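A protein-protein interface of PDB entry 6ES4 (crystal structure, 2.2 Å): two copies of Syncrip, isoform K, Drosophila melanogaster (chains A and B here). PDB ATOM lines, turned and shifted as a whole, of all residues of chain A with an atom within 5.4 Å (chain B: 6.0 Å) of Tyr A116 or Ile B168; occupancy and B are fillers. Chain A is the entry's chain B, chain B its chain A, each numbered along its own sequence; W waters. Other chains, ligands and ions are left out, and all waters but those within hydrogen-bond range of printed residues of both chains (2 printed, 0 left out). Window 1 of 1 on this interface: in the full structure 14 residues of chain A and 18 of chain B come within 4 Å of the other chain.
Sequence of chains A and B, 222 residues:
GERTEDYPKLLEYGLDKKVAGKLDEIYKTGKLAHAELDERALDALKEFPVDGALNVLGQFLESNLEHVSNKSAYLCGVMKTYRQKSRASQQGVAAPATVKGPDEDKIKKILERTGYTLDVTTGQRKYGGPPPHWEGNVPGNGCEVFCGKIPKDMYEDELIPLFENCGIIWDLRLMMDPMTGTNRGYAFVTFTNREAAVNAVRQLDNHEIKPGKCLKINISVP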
ATOM      1  N   LEU A 111       2.245   3.986 -32.363  1.00  0.00           N
ATOM      2  CA  LEU A 111       3.554   3.772 -31.754  1.00  0.00           C
ATOM      3  C   LEU A 111       4.675   4.406 -32.583  1.00  0.00           C
ATOM      4  O   LEU A 111       5.632   4.942 -32.032  1.00  0.00           O
ATOM      5  CB  LEU A 111       3.823   2.276 -31.562  1.00  0.00           C
ATOM      6  CG  LEU A 111       2.927   1.544 -30.553  1.00  0.00           C
ATOM      7  CD1 LEU A 111       3.426   0.124 -30.322  1.00  0.00           C
ATOM      8  CD2 LEU A 111       2.822   2.303 -29.231  1.00  0.00           C
ATOM      9  N   ARG A 113       4.508   7.131 -34.498  1.00  0.00           N
ATOM     10  CA  ARG A 113       4.473   8.587 -34.522  1.00  0.00           C
ATOM     11  C   ARG A 113       4.730   9.231 -33.161  1.00  0.00           C
ATOM     12  O   ARG A 113       5.103  10.401 -33.089  1.00  0.00           O
ATOM     13  CB  ARG A 113       3.132   9.047 -35.091  1.00  0.00           C
ATOM     14  CG  ARG A 113       2.978   8.645 -36.553  1.00  0.00           C
ATOM     15  CD  ARG A 113       1.540   8.671 -37.033  1.00  0.00           C
ATOM     16  NE  ARG A 113       1.415   8.006 -38.328  1.00  0.00           N
ATOM     17  CZ  ARG A 113       0.288   7.932 -39.028  1.00  0.00           C
ATOM     18  NH1 ARG A 113       0.274   7.306 -40.198  1.00  0.00           N
ATOM     19  NH2 ARG A 113      -0.825   8.483 -38.559  1.00  0.00           N
ATOM     20  N   THR A 114       4.546   8.472 -32.084  1.00  0.00           N
ATOM     21  CA  THR A 114       4.811   8.999 -30.749  1.00  0.00           C
ATOM     22  C   THR A 114       6.106   8.421 -30.186  1.00  0.00           C
ATOM     23  O   THR A 114       6.768   9.045 -29.356  1.00  0.00           O
ATOM     24  CB  THR A 114       3.656   8.698 -29.774  1.00  0.00           C
ATOM     25  OG1 THR A 114       3.604   7.291 -29.499  1.00  0.00           O
ATOM     26  CG2 THR A 114       2.333   9.143 -30.370  1.00  0.00           C
ATOM     27  N   GLY A 115       6.463   7.224 -30.644  1.00  0.00           N
ATOM     28  CA  GLY A 115       7.656   6.545 -30.171  1.00  0.00           C
ATOM     29  C   GLY A 115       7.448   5.868 -28.828  1.00  0.00           C
ATOM     30  O   GLY A 115       8.385   5.317 -28.249  1.00  0.00           O
ATOM     31  N   TYR A 116       6.214   5.907 -28.334  1.00  0.00           N
ATOM     32  CA  TYR A 116       5.884   5.339 -27.026  1.00  0.00           C
ATOM     33  C   TYR A 116       6.013   3.822 -26.992  1.00  0.00           C
ATOM     34  O   TYR A 116       5.753   3.143 -27.985  1.00  0.00           O
ATOM     35  CB  TYR A 116       4.461   5.721 -26.622  1.00  0.00           C
ATOM     36  CG  TYR A 116       4.314   7.096 -26.015  1.00  0.00           C
ATOM     37  CD1 TYR A 116       4.999   8.185 -26.532  1.00  0.00           C
ATOM     38  CD2 TYR A 116       3.459   7.311 -24.941  1.00  0.00           C
ATOM     39  CE1 TYR A 116       4.856   9.441 -25.982  1.00  0.00           C
ATOM     40  CE2 TYR A 116       3.305   8.569 -24.388  1.00  0.00           C
ATOM     41  CZ  TYR A 116       4.009   9.629 -24.911  1.00  0.00           C
ATOM     42  OH  TYR A 116       3.863  10.886 -24.367  1.00  0.00           O
ATOM     43  N   THR A 117       6.400   3.295 -25.836  1.00  0.00           N
ATOM     44  CA  THR A 117       6.406   1.856 -25.629  1.00  0.00           C
ATOM     45  C   THR A 117       4.985   1.338 -25.430  1.00  0.00           C
ATOM     46  O   THR A 117       4.108   2.057 -24.952  1.00  0.00           O
ATOM     47  CB  THR A 117       7.256   1.451 -24.404  1.00  0.00           C
ATOM     48  OG1 THR A 117       6.719   2.060 -23.221  1.00  0.00           O
ATOM     49  CG2 THR A 117       8.706   1.880 -24.585  1.00  0.00           C
ATOM     50  N   LEU A 118       4.767   0.088 -25.815  1.00  0.00           N
ATOM     51  CA  LEU A 118       3.540  -0.622 -25.492  1.00  0.00           C
ATOM     52  C   LEU A 118       3.920  -1.956 -24.865  1.00  0.00           C
ATOM     53  O   LEU A 118       4.627  -2.752 -25.479  1.00  0.00           O
ATOM     54  CB  LEU A 118       2.679  -0.838 -26.736  1.00  0.00           C
ATOM     55  CG  LEU A 118       1.378  -1.611 -26.510  1.00  0.00           C
ATOM     56  CD1 LEU A 118       0.448  -0.844 -25.574  1.00  0.00           C
ATOM     57  CD2 LEU A 118       0.691  -1.916 -27.834  1.00  0.00           C
ATOM     58  N   TYR A 127       0.514   1.695 -22.140  1.00  0.00           N
ATOM     59  CA  TYR A 127       1.020   2.595 -23.167  1.00  0.00           C
ATOM     60  C   TYR A 127       1.892   3.666 -22.518  1.00  0.00           C
ATOM     61  O   TYR A 127       1.444   4.377 -21.621  1.00  0.00           O
ATOM     62  CB  TYR A 127      -0.155   3.210 -23.931  1.00  0.00           C
ATOM     63  CG  TYR A 127       0.193   4.292 -24.924  1.00  0.00           C
ATOM     64  CD1 TYR A 127       0.820   3.987 -26.126  1.00  0.00           C
ATOM     65  CD2 TYR A 127      -0.146   5.616 -24.678  1.00  0.00           C
ATOM     66  CE1 TYR A 127       1.121   4.975 -27.045  1.00  0.00           C
ATOM     67  CE2 TYR A 127       0.151   6.613 -25.591  1.00  0.00           C
ATOM     68  CZ  TYR A 127       0.786   6.287 -26.774  1.00  0.00           C
ATOM     69  OH  TYR A 127       1.085   7.275 -27.687  1.00  0.00           O
ATOM     70  N   GLY A 128       3.145   3.764 -22.954  1.00  0.00           N
ATOM     71  CA  GLY A 128       4.078   4.717 -22.379  1.00  0.00           C
ATOM     72  C   GLY A 128       4.438   4.391 -20.940  1.00  0.00           C
ATOM     73  O   GLY A 128       4.606   3.225 -20.583  1.00  0.00           O
ATOM     74  N   GLY A 129       4.560   5.425 -20.112  1.00  0.00           N
ATOM     75  CA  GLY A 129       4.868   5.254 -18.702  1.00  0.00           C
ATOM     76  C   GLY A 129       6.214   4.614 -18.410  1.00  0.00           C
ATOM     77  O   GLY A 129       6.278   3.451 -17.997  1.00  0.00           O
ATOM     78  N   PRO A 131       6.955   8.127 -21.060  1.00  0.00           N
ATOM     79  CA  PRO A 131       7.161   8.472 -22.470  1.00  0.00           C
ATOM     80  C   PRO A 131       8.652   8.449 -22.789  1.00  0.00           C
ATOM     81  O   PRO A 131       9.463   8.406 -21.862  1.00  0.00           O
ATOM     82  CB  PRO A 131       6.600   9.894 -22.579  1.00  0.00           C
ATOM     83  CG  PRO A 131       5.737  10.072 -21.376  1.00  0.00           C
ATOM     84  CD  PRO A 131       6.358   9.238 -20.305  1.00  0.00           C
ATOM     85  N   PRO A 132       9.019   8.470 -24.078  1.00  0.00           N
ATOM     86  CA  PRO A 132      10.442   8.604 -24.398  1.00  0.00           C
ATOM     87  C   PRO A 132      10.979   9.948 -23.921  1.00  0.00           C
ATOM     88  O   PRO A 132      10.249  10.938 -23.968  1.00  0.00           O
ATOM     89  CB  PRO A 132      10.476   8.514 -25.930  1.00  0.00           C
ATOM     90  CG  PRO A 132       9.198   7.849 -26.311  1.00  0.00           C
ATOM     91  CD  PRO A 132       8.195   8.284 -25.284  1.00  0.00           C
ATOM     92  N   ILE A 168      -1.211  15.867 -23.046  1.00  0.00           N
ATOM     93  CA  ILE A 168      -0.161  14.910 -23.372  1.00  0.00           C
ATOM     94  C   ILE A 168      -0.190  13.710 -22.435  1.00  0.00           C
ATOM     95  O   ILE A 168       0.035  13.829 -21.232  1.00  0.00           O
ATOM     96  CB  ILE A 168       1.222  15.569 -23.336  1.00  0.00           C
ATOM     97  CG1 ILE A 168       1.245  16.753 -24.309  1.00  0.00           C
ATOM     98  CG2 ILE A 168       2.309  14.551 -23.693  1.00  0.00           C
ATOM     99  CD1 ILE A 168       2.534  17.522 -24.315  1.00  0.00           C
ATOM    100  N   ILE A 169      -0.493  12.552 -23.008  1.00  0.00           N
ATOM    101  CA  ILE A 169      -0.541  11.314 -22.253  1.00  0.00           C
ATOM    102  C   ILE A 169       0.850  10.959 -21.744  1.00  0.00           C
ATOM    103  O   ILE A 169       1.802  10.878 -22.519  1.00  0.00           O
ATOM    104  CB  ILE A 169      -1.098  10.160 -23.112  1.00  0.00           C
ATOM    105  CG1 ILE A 169      -2.522  10.482 -23.576  1.00  0.00           C
ATOM    106  CG2 ILE A 169      -1.059   8.847 -22.342  1.00  0.00           C
ATOM    107  CD1 ILE A 169      -3.124   9.440 -24.492  1.00  0.00           C
ATOM    108  N   TRP A 170       0.972  10.777 -20.434  1.00  0.00           N
ATOM    109  CA  TRP A 170       2.215  10.281 -19.863  1.00  0.00           C
ATOM    110  C   TRP A 170       2.181   8.756 -19.873  1.00  0.00           C
ATOM    111  O   TRP A 170       3.144   8.103 -20.277  1.00  0.00           O
ATOM    112  CB  TRP A 170       2.428  10.813 -18.446  1.00  0.00           C
ATOM    113  CG  TRP A 170       3.788  10.506 -17.900  1.00  0.00           C
ATOM    114  CD1 TRP A 170       4.924  11.239 -18.075  1.00  0.00           C
ATOM    115  CD2 TRP A 170       4.157   9.381 -17.090  1.00  0.00           C
ATOM    116  NE1 TRP A 170       5.980  10.642 -17.426  1.00  0.00           N
ATOM    117  CE2 TRP A 170       5.534   9.499 -16.813  1.00  0.00           C
ATOM    118  CE3 TRP A 170       3.456   8.287 -16.569  1.00  0.00           C
ATOM    119  CZ2 TRP A 170       6.226   8.566 -16.040  1.00  0.00           C
ATOM    120  CZ3 TRP A 170       4.144   7.361 -15.801  1.00  0.00           C
ATOM    121  CH2 TRP A 170       5.514   7.506 -15.544  1.00  0.00           C
ATOM    122  N   TYR B 116       3.702  23.643 -22.197  1.00  0.00           N
ATOM    123  CA  TYR B 116       4.794  24.149 -23.034  1.00  0.00           C
ATOM    124  C   TYR B 116       5.015  25.643 -22.830  1.00  0.00           C
ATOM    125  O   TYR B 116       4.079  26.381 -22.529  1.00  0.00           O
ATOM    126  CB  TYR B 116       4.516  23.895 -24.515  1.00  0.00           C
ATOM    127  CG  TYR B 116       4.850  22.509 -25.028  1.00  0.00           C
ATOM    128  CD1 TYR B 116       4.564  21.381 -24.276  1.00  0.00           C
ATOM    129  CD2 TYR B 116       5.413  22.334 -26.288  1.00  0.00           C
ATOM    130  CE1 TYR B 116       4.851  20.116 -24.750  1.00  0.00           C
ATOM    131  CE2 TYR B 116       5.702  21.073 -26.773  1.00  0.00           C
ATOM    132  CZ  TYR B 116       5.415  19.967 -25.992  1.00  0.00           C
ATOM    133  OH  TYR B 116       5.691  18.706 -26.451  1.00  0.00           O
ATOM    134  N   PHE B 163      -0.738  20.481 -36.308  1.00  0.00           N
ATOM    135  CA  PHE B 163       0.407  19.574 -36.343  1.00  0.00           C
ATOM    136  C   PHE B 163       0.398  18.571 -35.186  1.00  0.00           C
ATOM    137  O   PHE B 163       1.075  17.546 -35.246  1.00  0.00           O
ATOM    138  CB  PHE B 163       1.711  20.379 -36.366  1.00  0.00           C
ATOM    139  CG  PHE B 163       1.951  21.083 -37.681  1.00  0.00           C
ATOM    140  CD1 PHE B 163       2.385  20.373 -38.790  1.00  0.00           C
ATOM    141  CD2 PHE B 163       1.713  22.439 -37.814  1.00  0.00           C
ATOM    142  CE1 PHE B 163       2.591  21.006 -40.005  1.00  0.00           C
ATOM    143  CE2 PHE B 163       1.915  23.080 -39.028  1.00  0.00           C
ATOM    144  CZ  PHE B 163       2.355  22.363 -40.124  1.00  0.00           C
ATOM    145  N   GLU B 164      -0.389  18.848 -34.151  1.00  0.00           N
ATOM    146  CA  GLU B 164      -0.524  17.922 -33.026  1.00  0.00           C
ATOM    147  C   GLU B 164      -1.120  16.571 -33.434  1.00  0.00           C
ATOM    148  O   GLU B 164      -0.874  15.560 -32.780  1.00  0.00           O
ATOM    149  CB  GLU B 164      -1.378  18.542 -31.919  1.00  0.00           C
ATOM    150  CG  GLU B 164      -0.586  19.313 -30.879  1.00  0.00           C
ATOM    151  CD  GLU B 164      -1.470  19.882 -29.782  1.00  0.00           C
ATOM    152  OE1 GLU B 164      -2.666  20.124 -30.046  1.00  0.00           O
ATOM    153  OE2 GLU B 164      -0.969  20.082 -28.655  1.00  0.00           O
ATOM    154  N   CME B 166      -0.290  14.883 -35.955  1.00  0.00           N
ATOM    155  CA  CME B 166       0.693  14.155 -36.740  1.00  0.00           C
ATOM    156  CB  CME B 166       1.551  15.053 -37.641  1.00  0.00           C
ATOM    157  SG  CME B 166       0.595  15.997 -38.775  1.00  0.00           S
ATOM    158  SD  CME B 166      -0.455  14.570 -39.911  1.00  0.00           S
ATOM    159  CE  CME B 166      -2.064  15.229 -40.171  1.00  0.00           C
ATOM    160  CZ  CME B 166      -3.156  14.470 -39.454  1.00  0.00           C
ATOM    161  OH  CME B 166      -4.289  15.324 -39.442  1.00  0.00           O
ATOM    162  C   CME B 166       1.659  13.363 -35.870  1.00  0.00           C
ATOM    163  O   CME B 166       2.243  12.340 -36.239  1.00  0.00           O
ATOM    164  N   GLY B 167       1.843  13.875 -34.661  1.00  0.00           N
ATOM    165  CA  GLY B 167       2.783  13.303 -33.718  1.00  0.00           C
ATOM    166  C   GLY B 167       2.960  14.251 -32.551  1.00  0.00           C
ATOM    167  O   GLY B 167       2.109  15.107 -32.311  1.00  0.00           O
ATOM    168  N   ILE B 168       4.062  14.109 -31.827  1.00  0.00           N
ATOM    169  CA  ILE B 168       4.322  14.978 -30.689  1.00  0.00           C
ATOM    170  C   ILE B 168       5.233  16.125 -31.091  1.00  0.00           C
ATOM    171  O   ILE B 168       6.363  15.909 -31.531  1.00  0.00           O
ATOM    172  CB  ILE B 168       4.960  14.211 -29.515  1.00  0.00           C
ATOM    173  CG1 ILE B 168       4.120  12.984 -29.168  1.00  0.00           C
ATOM    174  CG2 ILE B 168       5.127  15.130 -28.297  1.00  0.00           C
ATOM    175  CD1 ILE B 168       4.678  12.187 -28.033  1.00  0.00           C
ATOM    176  N   ILE B 169       4.731  17.345 -30.945  1.00  0.00           N
ATOM    177  CA  ILE B 169       5.513  18.530 -31.269  1.00  0.00           C
ATOM    178  C   ILE B 169       6.603  18.750 -30.228  1.00  0.00           C
ATOM    179  O   ILE B 169       6.325  18.799 -29.028  1.00  0.00           O
ATOM    180  CB  ILE B 169       4.629  19.790 -31.352  1.00  0.00           C
ATOM    181  CG1 ILE B 169       3.541  19.609 -32.414  1.00  0.00           C
ATOM    182  CG2 ILE B 169       5.487  21.023 -31.635  1.00  0.00           C
ATOM    183  CD1 ILE B 169       2.590  20.790 -32.539  1.00  0.00           C
ATOM    184  N   TRP B 170       7.843  18.868 -30.692  1.00  0.00           N
ATOM    185  CA  TRP B 170       8.960  19.190 -29.811  1.00  0.00           C
ATOM    186  C   TRP B 170       9.126  20.703 -29.778  1.00  0.00           C
ATOM    187  O   TRP B 170       9.296  21.295 -28.709  1.00  0.00           O
ATOM    188  CB  TRP B 170      10.246  18.507 -30.277  1.00  0.00           C
ATOM    189  CG  TRP B 170      11.393  18.629 -29.310  1.00  0.00           C
ATOM    190  CD1 TRP B 170      11.679  17.795 -28.268  1.00  0.00           C
ATOM    191  CD2 TRP B 170      12.409  19.639 -29.307  1.00  0.00           C
ATOM    192  NE1 TRP B 170      12.810  18.224 -27.612  1.00  0.00           N
ATOM    193  CE2 TRP B 170      13.279  19.353 -28.231  1.00  0.00           C
ATOM    194  CE3 TRP B 170      12.671  20.758 -30.107  1.00  0.00           C
ATOM    195  CZ2 TRP B 170      14.391  20.146 -27.934  1.00  0.00           C
ATOM    196  CZ3 TRP B 170      13.777  21.544 -29.813  1.00  0.00           C
ATOM    197  CH2 TRP B 170      14.623  21.232 -28.735  1.00  0.00           C
ATOM    198  N   THR B 190       9.252  20.934 -35.368  1.00  0.00           N
ATOM    199  CA  THR B 190      10.046  19.755 -35.041  1.00  0.00           C
ATOM    200  C   THR B 190       9.225  18.772 -34.218  1.00  0.00           C
ATOM    201  O   THR B 190       8.634  19.140 -33.203  1.00  0.00           O
ATOM    202  CB  THR B 190      11.324  20.117 -34.263  1.00  0.00           C
ATOM    203  OG1 THR B 190      12.078  21.087 -35.002  1.00  0.00           O
ATOM    204  CG2 THR B 190      12.184  18.882 -34.025  1.00  0.00           C
ATOM    205  N   PHE B 191       9.181  17.525 -34.670  1.00  0.00           N
ATOM    206  CA  PHE B 191       8.508  16.469 -33.929  1.00  0.00           C
ATOM    207  C   PHE B 191       9.527  15.660 -33.139  1.00  0.00           C
ATOM    208  O   PHE B 191      10.729  15.863 -33.294  1.00  0.00           O
ATOM    209  CB  PHE B 191       7.719  15.573 -34.879  1.00  0.00           C
ATOM    210  CG  PHE B 191       6.576  16.276 -35.555  1.00  0.00           C
ATOM    211  CD1 PHE B 191       5.336  16.358 -34.937  1.00  0.00           C
ATOM    212  CD2 PHE B 191       6.740  16.857 -36.801  1.00  0.00           C
ATOM    213  CE1 PHE B 191       4.276  17.004 -35.553  1.00  0.00           C
ATOM    214  CE2 PHE B 191       5.682  17.508 -37.425  1.00  0.00           C
ATOM    215  CZ  PHE B 191       4.450  17.583 -36.797  1.00  0.00           C
ATOM    216  N   THR B 192       9.053  14.750 -32.294  1.00  0.00           N
ATOM    217  CA  THR B 192       9.955  13.989 -31.437  1.00  0.00           C
ATOM    218  C   THR B 192      10.634  12.841 -32.185  1.00  0.00           C
ATOM    219  O   THR B 192      11.642  12.318 -31.724  1.00  0.00           O
ATOM    220  CB  THR B 192       9.225  13.430 -30.199  1.00  0.00           C
ATOM    221  OG1 THR B 192       8.121  12.619 -30.611  1.00  0.00           O
ATOM    222  CG2 THR B 192       8.718  14.565 -29.317  1.00  0.00           C
ATOM    223  N   ASN B 193      10.083  12.445 -33.330  1.00  0.00           N
ATOM    224  CA  ASN B 193      10.778  11.504 -34.213  1.00  0.00           C
ATOM    225  C   ASN B 193      10.503  11.816 -35.687  1.00  0.00           C
ATOM    226  O   ASN B 193       9.699  12.694 -36.007  1.00  0.00           O
ATOM    227  CB  ASN B 193      10.404  10.050 -33.879  1.00  0.00           C
ATOM    228  CG  ASN B 193       8.915   9.763 -34.016  1.00  0.00           C
ATOM    229  OD1 ASN B 193       8.265  10.190 -34.970  1.00  0.00           O
ATOM    230  ND2 ASN B 193       8.370   9.018 -33.058  1.00  0.00           N
ATOM    231  N   ALA B 196       6.898  10.956 -37.420  1.00  0.00           N
ATOM    232  CA  ALA B 196       5.906  12.010 -37.257  1.00  0.00           C
ATOM    233  C   ALA B 196       6.110  13.101 -38.302  1.00  0.00           C
ATOM    234  O   ALA B 196       5.152  13.566 -38.914  1.00  0.00           O
ATOM    235  CB  ALA B 196       5.977  12.592 -35.854  1.00  0.00           C
HETATM  236  O   HOH W   1       6.361  12.576 -32.564  1.00  0.00           O
HETATM  237  O   HOH W   2       8.270  10.893 -28.325  1.00  0.00           O
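The backbone NH (N) of Thr B192 sits at hydrogen-bond distance from the backbone carbonyl oxygen (O) of Ile B168 (3.0 Å).
The side-chain hydroxyl (OG1) of Thr A114 is in hydrogen-bond range of the side-chain hydroxyl (OH) of Tyr A127, at 3.1 Å.
N of Tyr A116 lies close to OG1 of Thr A114 (3.2 Å).
The side-chain hydroxyl (OH) of Tyr B116 sits at hydrogen-bond distance from the backbone carbonyl oxygen (O) of Ile B169, 2.7 Å away.
The side-chain hydroxyl (OH) of Tyr A116 is in hydrogen-bond range of the backbone carbonyl oxygen (O) of Ile A169.
The side-chain amide oxygen of Asn B193 sits at hydrogen-bond distance from the backbone NH of Ala B196, at 2.9 Å.
CME B166 touches Arg A113.
O of Arg A113 touches CA of Gly B167, 3.8 Å away.
ND2 of Asn B193 touches O of Arg A113, 3.5 Å away.
Arg A113 touches Ala B196 (O to CB, 3.6 Å).
Thr A114 touches Ile B168.
Asn B193 touches Thr A114.
Asn B193 touches Gly A115 (ND2 to N, 3.6 Å).
CE1 of Tyr A116 touches CD1 of Ile B168 (3.4 Å).
Ile A168 touches Tyr B116 (CD1 to CE1, 3.5 Å).
Of chain B, only Ile B168 comes within 4 Å of Tyr A116.
Of the printed residues of chain A, Ile B168 touches Thr A114 and Tyr A116.
Printed residues of chain B within 4 Å of Ile A168: Tyr B116 (3.5 Å).
Printed residues of chain A within 4 Å of Asn B193: Arg A113 (3.5 Å), Thr A114 (3.7 Å) and Gly A115 (3.6 Å).
The nearest printed residue of chain B that does not touch Tyr A116 is Asn B193 (6.1 Å).
The nearest printed residue of chain A that does not touch Tyr B116 is Tyr A116 (8.3 Å).
Of the 15 printed residues of chain A, 5 touch a printed residue of chain B.
Printed residues of chain A that touch a printed residue of chain B: Arg A113, Thr A114, Gly A115, Tyr A116 and Ile A168.
Hydrophobic or aromatic side chains of chain A that line the printed part of chain B: Tyr A116 and Ile A168.
Of the 13 printed residues of chain B, 6 touch a printed residue of chain A.
Printed residues of chain B that touch a printed residue of chain A: Tyr B116, CME B166, Gly B167, Ile B168, Asn B193 and Ala B196.
Among the printed residues, no Asp or Glu carboxylate lies within 4 Å of a Lys or Arg side-chain nitrogen of the other chain.
Tyr A116 touches Ile B168, and with the chains exchanged Ile A168 touches Tyr B116.
Positions printed for both chains: 116, 168, 169 and 170.
Water W1 lies within hydrogen-bond range of the backbone carbonyl oxygen of Arg A113 (2.6 Å), the side-chain hydroxyl of Thr B192 (2.6 Å) and the backbone NH of Ile B168 (2.9 Å).
Water W2 bridges the backbone carbonyl oxygen of Thr A114 (2.6 Å) and the side-chain hydroxyl of Thr B192 (2.9 Å).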
